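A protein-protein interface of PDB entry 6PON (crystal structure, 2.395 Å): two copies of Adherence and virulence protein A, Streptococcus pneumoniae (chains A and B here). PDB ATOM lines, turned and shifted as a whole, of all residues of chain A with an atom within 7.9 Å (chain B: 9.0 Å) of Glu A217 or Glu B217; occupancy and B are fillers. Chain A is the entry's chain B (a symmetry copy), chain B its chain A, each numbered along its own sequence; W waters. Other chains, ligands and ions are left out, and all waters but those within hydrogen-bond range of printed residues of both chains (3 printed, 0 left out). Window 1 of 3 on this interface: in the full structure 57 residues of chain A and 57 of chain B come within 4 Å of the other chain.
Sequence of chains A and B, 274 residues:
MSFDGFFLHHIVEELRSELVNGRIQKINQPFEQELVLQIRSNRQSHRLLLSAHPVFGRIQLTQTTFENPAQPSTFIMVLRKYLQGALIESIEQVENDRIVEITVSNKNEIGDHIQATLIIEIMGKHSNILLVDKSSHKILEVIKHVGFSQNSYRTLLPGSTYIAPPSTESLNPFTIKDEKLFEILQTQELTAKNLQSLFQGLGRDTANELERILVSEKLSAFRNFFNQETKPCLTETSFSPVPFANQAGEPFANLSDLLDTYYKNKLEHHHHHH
The side-chain amino group (NZ) of Lys B218 sits at hydrogen-bond distance from the backbone carbonyl oxygen (O) of Leu A185 (3.1 Å).
O of Leu B185 lies within hydrogen-bond range of NZ of Lys A218 (2.9 Å).
The backbone carbonyl oxygen (O) of Ile B213 sits at hydrogen-bond distance from the side-chain hydroxyl (OG) of Ser B216 (3.5 Å).
The backbone carbonyl oxygen of Arg B212 sits at hydrogen-bond distance from the side-chain hydroxyl of Ser B216 (3.4 Å).
Phe A182 touches Val B215 (O to CG1, 3.6 Å).
CB of Ser B216 touches CE2 of Phe A182, at 3.9 Å.
CG1 of Val B215 touches C of Leu A185, 3.9 Å away.
CD1 of Leu A185 touches CA of Leu B219, 3.4 Å away.
Glu A217 touches Glu B217.
Lys A218 touches Leu B214.
Lys A218 touches Lys B218.
Leu A219 touches Leu B185 (CA to CD1, 3.5 Å).
Ala A221 touches Glu B217 (CB to CG, 3.6 Å).
CD2 of Phe A222 touches CD2 of Leu B185, at 3.96 Å.
Printed residues of chain B within 4 Å of Phe A182: Val B215, Ser B216 and Leu B219.
No residue of chain B comes within 4 Å of Ser A216.
Of chain B, only Glu B217 (3.3 Å) and Ala B221 (3.5 Å) come within 4 Å of Glu A217.
Printed residues of chain B within 4 Å of Leu A219: Leu B185 (3.5 Å).
Asn A224 touches none of the printed residues of chain B.
Arg B212 touches none of the printed residues of chain A.
Of chain A, only Phe A182 (3.9 Å) comes within 4 Å of Ser B216.
Glu B217 touches just these residues of chain A: Glu A217 (3.3 Å) and Ala A221 (3.6 Å).
The nearest residue of chain B that does not touch Glu A217 is Lys B218 (4.2 Å).
The nearest printed residue of chain B that does not touch Phe A222 is Leu B210 (4.01 Å).
Hydrophobic or aromatic side chains of chain A that line the printed part of chain B: Phe A182, Leu A185, Leu A210, Ile A213, Leu A214, Val A215, Ala A221 and Phe A222.
Of the 18 printed residues of chain B, 10 touch a printed residue of chain A.
Hydrophobic or aromatic side chains of chain B within 4 Å of the printed part of chain A: Phe B182, Leu B185, Leu B214, Val B215, Leu B219, Ala B221 and Phe B222.
Among the printed residues, 18 pairs touch across the chains.
Among the printed residues, no Asp or Glu carboxylate lies within 4 Å of a Lys or Arg side-chain nitrogen of the other chain.
Phe A182 touches Val B215, and with the chains exchanged Val A215 touches Phe B182.
Phe A182 touches Leu B219, but with the chains exchanged Leu A219 does not touch Phe B182 (4.1 Å).
Leu A185 touches Val B215, but with the chains exchanged Val A215 does not touch Leu B185 (5.8 Å).
Glu A217 touches Ala B221, and with the chains exchanged Ala A221 touches Glu B217.
Of the 18 pairs that touch across the chains among the printed residues, 12 have their exchanged pair printed and touching as well.
Water W1 bridges OE2 of Glu B217 (2.6 Å) and OE1 of Glu A217 (2.7 Å).
Water W3 bridges NZ of Lys B218 (2.6 Å) and NZ of Lys A218 (2.8 Å).
Water W2 bridges the side-chain carboxylate (OE2) of Glu B217 and the side-chain amide nitrogen (ND2) of Asn A224.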
ATOM      1  N   PHE A 182      16.235  23.631  -0.148  1.00  0.00           N
ATOM      2  CA  PHE A 182      15.973  22.483  -1.012  1.00  0.00           C
ATOM      3  C   PHE A 182      14.866  21.611  -0.426  1.00  0.00           C
ATOM      4  O   PHE A 182      13.890  21.277  -1.108  1.00  0.00           O
ATOM      5  CB  PHE A 182      17.270  21.687  -1.201  1.00  0.00           C
ATOM      6  CG  PHE A 182      17.230  20.684  -2.315  1.00  0.00           C
ATOM      7  CD1 PHE A 182      16.672  19.424  -2.114  1.00  0.00           C
ATOM      8  CD2 PHE A 182      17.784  20.979  -3.551  1.00  0.00           C
ATOM      9  CE1 PHE A 182      16.649  18.484  -3.132  1.00  0.00           C
ATOM     10  CE2 PHE A 182      17.755  20.053  -4.580  1.00  0.00           C
ATOM     11  CZ  PHE A 182      17.189  18.802  -4.370  1.00  0.00           C
ATOM     12  N   LEU A 185      11.597  23.217  -0.888  1.00  0.00           N
ATOM     13  CA  LEU A 185      11.112  23.197  -2.257  1.00  0.00           C
ATOM     14  C   LEU A 185      10.805  21.784  -2.737  1.00  0.00           C
ATOM     15  O   LEU A 185       9.998  21.617  -3.656  1.00  0.00           O
ATOM     16  CB  LEU A 185      12.126  23.854  -3.188  1.00  0.00           C
ATOM     17  CG  LEU A 185      12.460  25.310  -2.919  1.00  0.00           C
ATOM     18  CD1 LEU A 185      13.688  25.685  -3.724  1.00  0.00           C
ATOM     19  CD2 LEU A 185      11.271  26.240  -3.244  1.00  0.00           C
ATOM     20  N   LEU A 210       6.290  35.006  -6.809  1.00  0.00           N
ATOM     21  CA  LEU A 210       7.164  33.885  -6.502  1.00  0.00           C
ATOM     22  C   LEU A 210       6.488  32.562  -6.839  1.00  0.00           C
ATOM     23  O   LEU A 210       7.092  31.698  -7.491  1.00  0.00           O
ATOM     24  CB  LEU A 210       7.586  33.923  -5.039  1.00  0.00           C
ATOM     25  CG  LEU A 210       8.663  32.902  -4.656  1.00  0.00           C
ATOM     26  CD1 LEU A 210       9.867  32.974  -5.596  1.00  0.00           C
ATOM     27  CD2 LEU A 210       9.098  33.040  -3.187  1.00  0.00           C
ATOM     28  N   GLU A 211       5.232  32.376  -6.402  1.00  0.00           N
ATOM     29  CA  GLU A 211       4.510  31.162  -6.768  1.00  0.00           C
ATOM     30  C   GLU A 211       4.530  30.957  -8.277  1.00  0.00           C
ATOM     31  O   GLU A 211       4.810  29.853  -8.760  1.00  0.00           O
ATOM     32  CB  GLU A 211       3.059  31.184  -6.267  1.00  0.00           C
ATOM     33  CG  GLU A 211       2.237  29.956  -6.785  1.00  0.00           C
ATOM     34  CD  GLU A 211       0.732  29.972  -6.444  1.00  0.00           C
ATOM     35  OE1 GLU A 211       0.297  30.640  -5.485  1.00  0.00           O
ATOM     36  OE2 GLU A 211      -0.031  29.275  -7.147  1.00  0.00           O
ATOM     37  N   ARG A 212       4.255  32.022  -9.040  1.00  0.00           N
ATOM     38  CA  ARG A 212       4.242  31.897 -10.492  1.00  0.00           C
ATOM     39  C   ARG A 212       5.615  31.529 -11.026  1.00  0.00           C
ATOM     40  O   ARG A 212       5.726  30.782 -12.004  1.00  0.00           O
ATOM     41  CB  ARG A 212       3.777  33.193 -11.142  1.00  0.00           C
ATOM     42  CG  ARG A 212       3.611  33.075 -12.641  1.00  0.00           C
ATOM     43  CD  ARG A 212       3.682  34.444 -13.303  1.00  0.00           C
ATOM     44  NE  ARG A 212       4.963  35.101 -13.039  1.00  0.00           N
ATOM     45  CZ  ARG A 212       6.066  34.907 -13.759  1.00  0.00           C
ATOM     46  NH1 ARG A 212       6.038  34.066 -14.790  1.00  0.00           N
ATOM     47  NH2 ARG A 212       7.196  35.536 -13.440  1.00  0.00           N
ATOM     48  N   ILE A 213       6.668  32.042 -10.395  1.00  0.00           N
ATOM     49  CA  ILE A 213       8.012  31.800 -10.890  1.00  0.00           C
ATOM     50  C   ILE A 213       8.377  30.338 -10.731  1.00  0.00           C
ATOM     51  O   ILE A 213       8.924  29.720 -11.650  1.00  0.00           O
ATOM     52  CB  ILE A 213       9.002  32.718 -10.163  1.00  0.00           C
ATOM     53  CG1 ILE A 213       8.881  34.131 -10.725  1.00  0.00           C
ATOM     54  CG2 ILE A 213      10.426  32.165 -10.235  1.00  0.00           C
ATOM     55  CD1 ILE A 213       9.757  35.147  -9.994  1.00  0.00           C
ATOM     56  N   LEU A 214       8.065  29.758  -9.571  1.00  0.00           N
ATOM     57  CA  LEU A 214       8.450  28.381  -9.308  1.00  0.00           C
ATOM     58  C   LEU A 214       7.637  27.422 -10.176  1.00  0.00           C
ATOM     59  O   LEU A 214       8.179  26.447 -10.707  1.00  0.00           O
ATOM     60  CB  LEU A 214       8.292  28.069  -7.813  1.00  0.00           C
ATOM     61  CG  LEU A 214       9.065  28.940  -6.820  1.00  0.00           C
ATOM     62  CD1 LEU A 214       8.503  28.875  -5.378  1.00  0.00           C
ATOM     63  CD2 LEU A 214      10.529  28.563  -6.821  1.00  0.00           C
ATOM     64  N   VAL A 215       6.341  27.704 -10.350  1.00  0.00           N
ATOM     65  CA  VAL A 215       5.511  26.946 -11.285  1.00  0.00           C
ATOM     66  C   VAL A 215       6.116  26.978 -12.682  1.00  0.00           C
ATOM     67  O   VAL A 215       6.392  25.934 -13.291  1.00  0.00           O
ATOM     68  CB  VAL A 215       4.075  27.494 -11.280  1.00  0.00           C
ATOM     69  CG1 VAL A 215       3.309  27.033 -12.520  1.00  0.00           C
ATOM     70  CG2 VAL A 215       3.369  27.060  -9.996  1.00  0.00           C
ATOM     71  N   SER A 216       6.366  28.178 -13.192  1.00  0.00           N
ATOM     72  CA  SER A 216       6.943  28.324 -14.521  1.00  0.00           C
ATOM     73  C   SER A 216       8.296  27.625 -14.631  1.00  0.00           C
ATOM     74  O   SER A 216       8.599  27.003 -15.653  1.00  0.00           O
ATOM     75  CB  SER A 216       7.059  29.810 -14.865  1.00  0.00           C
ATOM     76  OG  SER A 216       7.694  29.978 -16.120  1.00  0.00           O
ATOM     77  N   GLU A 217       9.123  27.711 -13.596  1.00  0.00           N
ATOM     78  CA  GLU A 217      10.440  27.085 -13.661  1.00  0.00           C
ATOM     79  C   GLU A 217      10.323  25.570 -13.682  1.00  0.00           C
ATOM     80  O   GLU A 217      11.095  24.889 -14.363  1.00  0.00           O
ATOM     81  CB  GLU A 217      11.290  27.523 -12.470  1.00  0.00           C
ATOM     82  CG  GLU A 217      12.723  27.008 -12.542  1.00  0.00           C
ATOM     83  CD  GLU A 217      13.422  27.484 -13.801  1.00  0.00           C
ATOM     84  OE1 GLU A 217      14.048  26.632 -14.476  1.00  0.00           O
ATOM     85  OE2 GLU A 217      13.312  28.701 -14.128  1.00  0.00           O
ATOM     86  N   LYS A 218       9.366  25.034 -12.928  1.00  0.00           N
ATOM     87  CA  LYS A 218       9.124  23.600 -12.913  1.00  0.00           C
ATOM     88  C   LYS A 218       8.824  23.078 -14.316  1.00  0.00           C
ATOM     89  O   LYS A 218       9.403  22.078 -14.758  1.00  0.00           O
ATOM     90  CB  LYS A 218       7.973  23.311 -11.960  1.00  0.00           C
ATOM     91  CG  LYS A 218       8.127  22.047 -11.192  1.00  0.00           C
ATOM     92  CD  LYS A 218       7.324  22.105  -9.907  1.00  0.00           C
ATOM     93  CE  LYS A 218       5.862  21.810 -10.147  1.00  0.00           C
ATOM     94  NZ  LYS A 218       5.097  21.940  -8.885  1.00  0.00           N
ATOM     95  N   LEU A 219       7.941  23.764 -15.044  1.00  0.00           N
ATOM     96  CA  LEU A 219       7.574  23.336 -16.390  1.00  0.00           C
ATOM     97  C   LEU A 219       8.761  23.412 -17.335  1.00  0.00           C
ATOM     98  O   LEU A 219       8.998  22.494 -18.136  1.00  0.00           O
ATOM     99  CB  LEU A 219       6.424  24.203 -16.906  1.00  0.00           C
ATOM    100  CG  LEU A 219       5.940  23.785 -18.254  1.00  0.00           C
ATOM    101  CD1 LEU A 219       4.527  23.360 -18.262  1.00  0.00           C
ATOM    102  CD2 LEU A 219       6.169  24.867 -19.256  1.00  0.00           C
ATOM    103  N   SER A 220       9.526  24.492 -17.233  1.00  0.00           N
ATOM    104  CA  SER A 220      10.681  24.695 -18.095  1.00  0.00           C
ATOM    105  C   SER A 220      11.748  23.643 -17.836  1.00  0.00           C
ATOM    106  O   SER A 220      12.392  23.150 -18.768  1.00  0.00           O
ATOM    107  CB  SER A 220      11.230  26.105 -17.862  1.00  0.00           C
ATOM    108  OG  SER A 220      12.507  26.255 -18.454  1.00  0.00           O
ATOM    109  N   ALA A 221      11.942  23.279 -16.569  1.00  0.00           N
ATOM    110  CA  ALA A 221      12.910  22.240 -16.261  1.00  0.00           C
ATOM    111  C   ALA A 221      12.448  20.906 -16.808  1.00  0.00           C
ATOM    112  O   ALA A 221      13.259  20.126 -17.317  1.00  0.00           O
ATOM    113  CB  ALA A 221      13.139  22.168 -14.756  1.00  0.00           C
ATOM    114  N   PHE A 222      11.143  20.638 -16.728  1.00  0.00           N
ATOM    115  CA  PHE A 222      10.606  19.384 -17.237  1.00  0.00           C
ATOM    116  C   PHE A 222      10.836  19.281 -18.738  1.00  0.00           C
ATOM    117  O   PHE A 222      11.323  18.257 -19.235  1.00  0.00           O
ATOM    118  CB  PHE A 222       9.112  19.278 -16.899  1.00  0.00           C
ATOM    119  CG  PHE A 222       8.485  17.933 -17.261  1.00  0.00           C
ATOM    120  CD1 PHE A 222       8.188  17.612 -18.583  1.00  0.00           C
ATOM    121  CD2 PHE A 222       8.183  17.001 -16.275  1.00  0.00           C
ATOM    122  CE1 PHE A 222       7.613  16.398 -18.906  1.00  0.00           C
ATOM    123  CE2 PHE A 222       7.604  15.791 -16.590  1.00  0.00           C
ATOM    124  CZ  PHE A 222       7.322  15.484 -17.896  1.00  0.00           C
ATOM    125  N   ARG A 223      10.514  20.353 -19.469  1.00  0.00           N
ATOM    126  CA  ARG A 223      10.718  20.381 -20.913  1.00  0.00           C
ATOM    127  C   ARG A 223      12.186  20.190 -21.272  1.00  0.00           C
ATOM    128  O   ARG A 223      12.520  19.413 -22.174  1.00  0.00           O
ATOM    129  CB  ARG A 223      10.196  21.697 -21.490  1.00  0.00           C
ATOM    130  CG  ARG A 223       8.703  21.822 -21.445  1.00  0.00           C
ATOM    131  CD  ARG A 223       8.041  20.629 -22.145  1.00  0.00           C
ATOM    132  NE  ARG A 223       6.635  20.890 -22.471  1.00  0.00           N
ATOM    133  CZ  ARG A 223       5.760  19.967 -22.859  1.00  0.00           C
ATOM    134  NH1 ARG A 223       6.112  18.685 -22.965  1.00  0.00           N
ATOM    135  NH2 ARG A 223       4.523  20.323 -23.144  1.00  0.00           N
ATOM    136  N   ASN A 224      13.078  20.889 -20.579  1.00  0.00           N
ATOM    137  CA  ASN A 224      14.495  20.772 -20.910  1.00  0.00           C
ATOM    138  C   ASN A 224      14.995  19.349 -20.695  1.00  0.00           C
ATOM    139  O   ASN A 224      15.742  18.815 -21.522  1.00  0.00           O
ATOM    140  CB  ASN A 224      15.325  21.749 -20.077  1.00  0.00           C
ATOM    141  CG  ASN A 224      15.144  23.194 -20.512  1.00  0.00           C
ATOM    142  OD1 ASN A 224      14.555  23.477 -21.565  1.00  0.00           O
ATOM    143  ND2 ASN A 224      15.667  24.124 -19.705  1.00  0.00           N
ATOM    144  N   PHE B 182       1.105  21.061 -17.764  1.00  0.00           N
ATOM    145  CA  PHE B 182       0.908  22.120 -16.786  1.00  0.00           C
ATOM    146  C   PHE B 182      -0.005  21.653 -15.657  1.00  0.00           C
ATOM    147  O   PHE B 182       0.306  21.830 -14.469  1.00  0.00           O
ATOM    148  CB  PHE B 182       0.352  23.363 -17.487  1.00  0.00           C
ATOM    149  CG  PHE B 182       0.316  24.579 -16.610  1.00  0.00           C
ATOM    150  CD1 PHE B 182       1.445  25.380 -16.468  1.00  0.00           C
ATOM    151  CD2 PHE B 182      -0.834  24.909 -15.898  1.00  0.00           C
ATOM    152  CE1 PHE B 182       1.428  26.503 -15.640  1.00  0.00           C
ATOM    153  CE2 PHE B 182      -0.866  26.025 -15.075  1.00  0.00           C
ATOM    154  CZ  PHE B 182       0.271  26.827 -14.946  1.00  0.00           C
ATOM    155  N   LEU B 185       1.816  19.149 -13.442  1.00  0.00           N
ATOM    156  CA  LEU B 185       2.895  19.724 -12.643  1.00  0.00           C
ATOM    157  C   LEU B 185       2.380  20.645 -11.533  1.00  0.00           C
ATOM    158  O   LEU B 185       3.000  20.736 -10.466  1.00  0.00           O
ATOM    159  CB  LEU B 185       3.871  20.483 -13.546  1.00  0.00           C
ATOM    160  CG  LEU B 185       4.692  19.690 -14.556  1.00  0.00           C
ATOM    161  CD1 LEU B 185       5.664  20.583 -15.275  1.00  0.00           C
ATOM    162  CD2 LEU B 185       5.459  18.595 -13.884  1.00  0.00           C
ATOM    163  N   GLU B 209      16.229  11.172 -10.800  1.00  0.00           N
ATOM    164  CA  GLU B 209      16.953  12.328 -11.312  1.00  0.00           C
ATOM    165  C   GLU B 209      15.997  13.435 -11.727  1.00  0.00           C
ATOM    166  O   GLU B 209      16.294  14.611 -11.519  1.00  0.00           O
ATOM    167  CB  GLU B 209      17.850  11.931 -12.484  1.00  0.00           C
ATOM    168  CG  GLU B 209      18.500  13.138 -13.158  1.00  0.00           C
ATOM    169  CD  GLU B 209      19.640  13.735 -12.351  1.00  0.00           C
ATOM    170  OE1 GLU B 209      19.919  13.247 -11.230  1.00  0.00           O
ATOM    171  OE2 GLU B 209      20.273  14.680 -12.855  1.00  0.00           O
ATOM    172  N   LEU B 210      14.837  13.082 -12.300  1.00  0.00           N
ATOM    173  CA  LEU B 210      13.877  14.112 -12.688  1.00  0.00           C
ATOM    174  C   LEU B 210      13.314  14.832 -11.466  1.00  0.00           C
ATOM    175  O   LEU B 210      13.160  16.063 -11.474  1.00  0.00           O
ATOM    176  CB  LEU B 210      12.752  13.502 -13.523  1.00  0.00           C
ATOM    177  CG  LEU B 210      11.611  14.450 -13.913  1.00  0.00           C
ATOM    178  CD1 LEU B 210      12.128  15.730 -14.529  1.00  0.00           C
ATOM    179  CD2 LEU B 210      10.600  13.774 -14.851  1.00  0.00           C
ATOM    180  N   GLU B 211      12.989  14.086 -10.410  1.00  0.00           N
ATOM    181  CA  GLU B 211      12.535  14.732  -9.185  1.00  0.00           C
ATOM    182  C   GLU B 211      13.580  15.713  -8.675  1.00  0.00           C
ATOM    183  O   GLU B 211      13.250  16.844  -8.310  1.00  0.00           O
ATOM    184  CB  GLU B 211      12.203  13.696  -8.101  1.00  0.00           C
ATOM    185  CG  GLU B 211      11.878  14.402  -6.772  1.00  0.00           C
ATOM    186  CD  GLU B 211      11.524  13.474  -5.614  1.00  0.00           C
ATOM    187  OE1 GLU B 211      11.597  12.229  -5.762  1.00  0.00           O
ATOM    188  OE2 GLU B 211      11.151  14.015  -4.548  1.00  0.00           O
ATOM    189  N   ARG B 212      14.850  15.302  -8.671  1.00  0.00           N
ATOM    190  CA  ARG B 212      15.918  16.163  -8.173  1.00  0.00           C
ATOM    191  C   ARG B 212      16.047  17.419  -9.023  1.00  0.00           C
ATOM    192  O   ARG B 212      16.127  18.538  -8.496  1.00  0.00           O
ATOM    193  CB  ARG B 212      17.229  15.373  -8.150  1.00  0.00           C
ATOM    194  CG  ARG B 212      18.449  16.089  -7.619  1.00  0.00           C
ATOM    195  CD  ARG B 212      19.742  15.356  -8.081  1.00  0.00           C
ATOM    196  NE  ARG B 212      20.039  15.686  -9.469  1.00  0.00           N
ATOM    197  CZ  ARG B 212      20.547  16.857  -9.855  1.00  0.00           C
ATOM    198  NH1 ARG B 212      20.838  17.781  -8.944  1.00  0.00           N
ATOM    199  NH2 ARG B 212      20.766  17.109 -11.141  1.00  0.00           N
ATOM    200  N   ILE B 213      16.072  17.244 -10.349  1.00  0.00           N
ATOM    201  CA  ILE B 213      16.195  18.356 -11.281  1.00  0.00           C
ATOM    202  C   ILE B 213      15.094  19.382 -11.047  1.00  0.00           C
ATOM    203  O   ILE B 213      15.343  20.596 -11.066  1.00  0.00           O
ATOM    204  CB  ILE B 213      16.169  17.823 -12.726  1.00  0.00           C
ATOM    205  CG1 ILE B 213      17.550  17.327 -13.138  1.00  0.00           C
ATOM    206  CG2 ILE B 213      15.688  18.911 -13.699  1.00  0.00           C
ATOM    207  CD1 ILE B 213      18.456  18.464 -13.616  1.00  0.00           C
ATOM    208  N   LEU B 214      13.854  18.916 -10.852  1.00  0.00           N
ATOM    209  CA  LEU B 214      12.748  19.843 -10.623  1.00  0.00           C
ATOM    210  C   LEU B 214      12.992  20.685  -9.370  1.00  0.00           C
ATOM    211  O   LEU B 214      12.764  21.900  -9.370  1.00  0.00           O
ATOM    212  CB  LEU B 214      11.430  19.062 -10.522  1.00  0.00           C
ATOM    213  CG  LEU B 214      10.960  18.359 -11.817  1.00  0.00           C
ATOM    214  CD1 LEU B 214       9.806  17.369 -11.606  1.00  0.00           C
ATOM    215  CD2 LEU B 214      10.590  19.390 -12.883  1.00  0.00           C
ATOM    216  N   VAL B 215      13.502  20.068  -8.304  1.00  0.00           N
ATOM    217  CA  VAL B 215      13.689  20.814  -7.070  1.00  0.00           C
ATOM    218  C   VAL B 215      14.876  21.767  -7.194  1.00  0.00           C
ATOM    219  O   VAL B 215      14.808  22.924  -6.756  1.00  0.00           O
ATOM    220  CB  VAL B 215      13.840  19.850  -5.883  1.00  0.00           C
ATOM    221  CG1 VAL B 215      14.003  20.630  -4.614  1.00  0.00           C
ATOM    222  CG2 VAL B 215      12.623  18.935  -5.782  1.00  0.00           C
ATOM    223  N   SER B 216      15.970  21.317  -7.820  1.00  0.00           N
ATOM    224  CA  SER B 216      17.153  22.171  -7.857  1.00  0.00           C
ATOM    225  C   SER B 216      16.985  23.322  -8.846  1.00  0.00           C
ATOM    226  O   SER B 216      17.615  24.375  -8.678  1.00  0.00           O
ATOM    227  CB  SER B 216      18.414  21.345  -8.165  1.00  0.00           C
ATOM    228  OG  SER B 216      18.406  20.798  -9.466  1.00  0.00           O
ATOM    229  N   GLU B 217      16.152  23.146  -9.878  1.00  0.00           N
ATOM    230  CA  GLU B 217      15.853  24.265 -10.766  1.00  0.00           C
ATOM    231  C   GLU B 217      14.936  25.271 -10.081  1.00  0.00           C
ATOM    232  O   GLU B 217      15.046  26.482 -10.321  1.00  0.00           O
ATOM    233  CB  GLU B 217      15.224  23.763 -12.069  1.00  0.00           C
ATOM    234  CG  GLU B 217      16.180  22.980 -12.990  1.00  0.00           C
ATOM    235  CD  GLU B 217      17.302  23.856 -13.545  1.00  0.00           C
ATOM    236  OE1 GLU B 217      18.418  23.857 -12.976  1.00  0.00           O
ATOM    237  OE2 GLU B 217      17.047  24.571 -14.541  1.00  0.00           O
ATOM    238  N   LYS B 218      14.031  24.787  -9.225  1.00  0.00           N
ATOM    239  CA  LYS B 218      13.227  25.700  -8.426  1.00  0.00           C
ATOM    240  C   LYS B 218      14.110  26.487  -7.476  1.00  0.00           C
ATOM    241  O   LYS B 218      13.914  27.693  -7.296  1.00  0.00           O
ATOM    242  CB  LYS B 218      12.137  24.939  -7.668  1.00  0.00           C
ATOM    243  CG  LYS B 218      10.933  24.582  -8.542  1.00  0.00           C
ATOM    244  CD  LYS B 218       9.768  23.959  -7.752  1.00  0.00           C
ATOM    245  CE  LYS B 218      10.167  22.624  -7.178  1.00  0.00           C
ATOM    246  NZ  LYS B 218       9.019  21.923  -6.540  1.00  0.00           N
ATOM    247  N   LEU B 219      15.126  25.828  -6.911  1.00  0.00           N
ATOM    248  CA  LEU B 219      16.070  26.505  -6.035  1.00  0.00           C
ATOM    249  C   LEU B 219      16.791  27.619  -6.771  1.00  0.00           C
ATOM    250  O   LEU B 219      16.930  28.740  -6.256  1.00  0.00           O
ATOM    251  CB  LEU B 219      17.070  25.493  -5.475  1.00  0.00           C
ATOM    252  CG  LEU B 219      17.915  25.979  -4.298  1.00  0.00           C
ATOM    253  CD1 LEU B 219      18.102  24.859  -3.325  1.00  0.00           C
ATOM    254  CD2 LEU B 219      19.279  26.480  -4.792  1.00  0.00           C
ATOM    255  N   SER B 220      17.260  27.318  -7.978  1.00  0.00           N
ATOM    256  CA  SER B 220      17.925  28.308  -8.809  1.00  0.00           C
ATOM    257  C   SER B 220      17.000  29.481  -9.110  1.00  0.00           C
ATOM    258  O   SER B 220      17.405  30.649  -9.013  1.00  0.00           O
ATOM    259  CB  SER B 220      18.392  27.635 -10.097  1.00  0.00           C
ATOM    260  OG  SER B 220      19.105  28.531 -10.911  1.00  0.00           O
ATOM    261  N   ALA B 221      15.750  29.186  -9.491  1.00  0.00           N
ATOM    262  CA  ALA B 221      14.783  30.243  -9.759  1.00  0.00           C
ATOM    263  C   ALA B 221      14.498  31.036  -8.503  1.00  0.00           C
ATOM    264  O   ALA B 221      14.268  32.251  -8.572  1.00  0.00           O
ATOM    265  CB  ALA B 221      13.481  29.654 -10.307  1.00  0.00           C
ATOM    266  N   PHE B 222      14.517  30.360  -7.350  1.00  0.00           N
ATOM    267  CA  PHE B 222      14.235  31.006  -6.072  1.00  0.00           C
ATOM    268  C   PHE B 222      15.303  32.036  -5.734  1.00  0.00           C
ATOM    269  O   PHE B 222      14.983  33.155  -5.322  1.00  0.00           O
ATOM    270  CB  PHE B 222      14.147  29.952  -4.975  1.00  0.00           C
ATOM    271  CG  PHE B 222      13.691  30.486  -3.636  1.00  0.00           C
ATOM    272  CD1 PHE B 222      14.581  31.141  -2.785  1.00  0.00           C
ATOM    273  CD2 PHE B 222      12.382  30.296  -3.212  1.00  0.00           C
ATOM    274  CE1 PHE B 222      14.156  31.620  -1.537  1.00  0.00           C
ATOM    275  CE2 PHE B 222      11.963  30.774  -1.988  1.00  0.00           C
ATOM    276  CZ  PHE B 222      12.849  31.435  -1.144  1.00  0.00           C
ATOM    277  N   ARG B 223      16.574  31.650  -5.871  1.00  0.00           N
ATOM    278  CA  ARG B 223      17.687  32.549  -5.574  1.00  0.00           C
ATOM    279  C   ARG B 223      17.658  33.763  -6.488  1.00  0.00           C
ATOM    280  O   ARG B 223      17.756  34.901  -6.022  1.00  0.00           O
ATOM    281  CB  ARG B 223      19.031  31.821  -5.727  1.00  0.00           C
ATOM    282  CG  ARG B 223      19.291  30.675  -4.771  1.00  0.00           C
ATOM    283  CD  ARG B 223      19.285  31.139  -3.307  1.00  0.00           C
ATOM    284  NE  ARG B 223      19.870  30.142  -2.413  1.00  0.00           N
ATOM    285  CZ  ARG B 223      19.688  30.106  -1.093  1.00  0.00           C
ATOM    286  NH1 ARG B 223      18.915  31.005  -0.490  1.00  0.00           N
ATOM    287  NH2 ARG B 223      20.278  29.163  -0.371  1.00  0.00           N
ATOM    288  N   ASN B 224      17.547  33.531  -7.801  1.00  0.00           N
ATOM    289  CA  ASN B 224      17.573  34.631  -8.759  1.00  0.00           C
ATOM    290  C   ASN B 224      16.505  35.667  -8.443  1.00  0.00           C
ATOM    291  O   ASN B 224      16.741  36.871  -8.582  1.00  0.00           O
ATOM    292  CB  ASN B 224      17.396  34.107 -10.189  1.00  0.00           C
ATOM    293  CG  ASN B 224      18.560  33.220 -10.650  1.00  0.00           C
ATOM    294  OD1 ASN B 224      19.600  33.124  -9.987  1.00  0.00           O
ATOM    295  ND2 ASN B 224      18.380  32.565 -11.797  1.00  0.00           N
HETATM  296  O   HOH W   1      16.615  27.074 -13.950  1.00  0.00           O
HETATM  297  O   HOH W   2      16.530  23.377 -16.929  1.00  0.00           O
HETATM  298  O   HOH W   3       6.550  22.850  -6.616  1.00  0.00           O
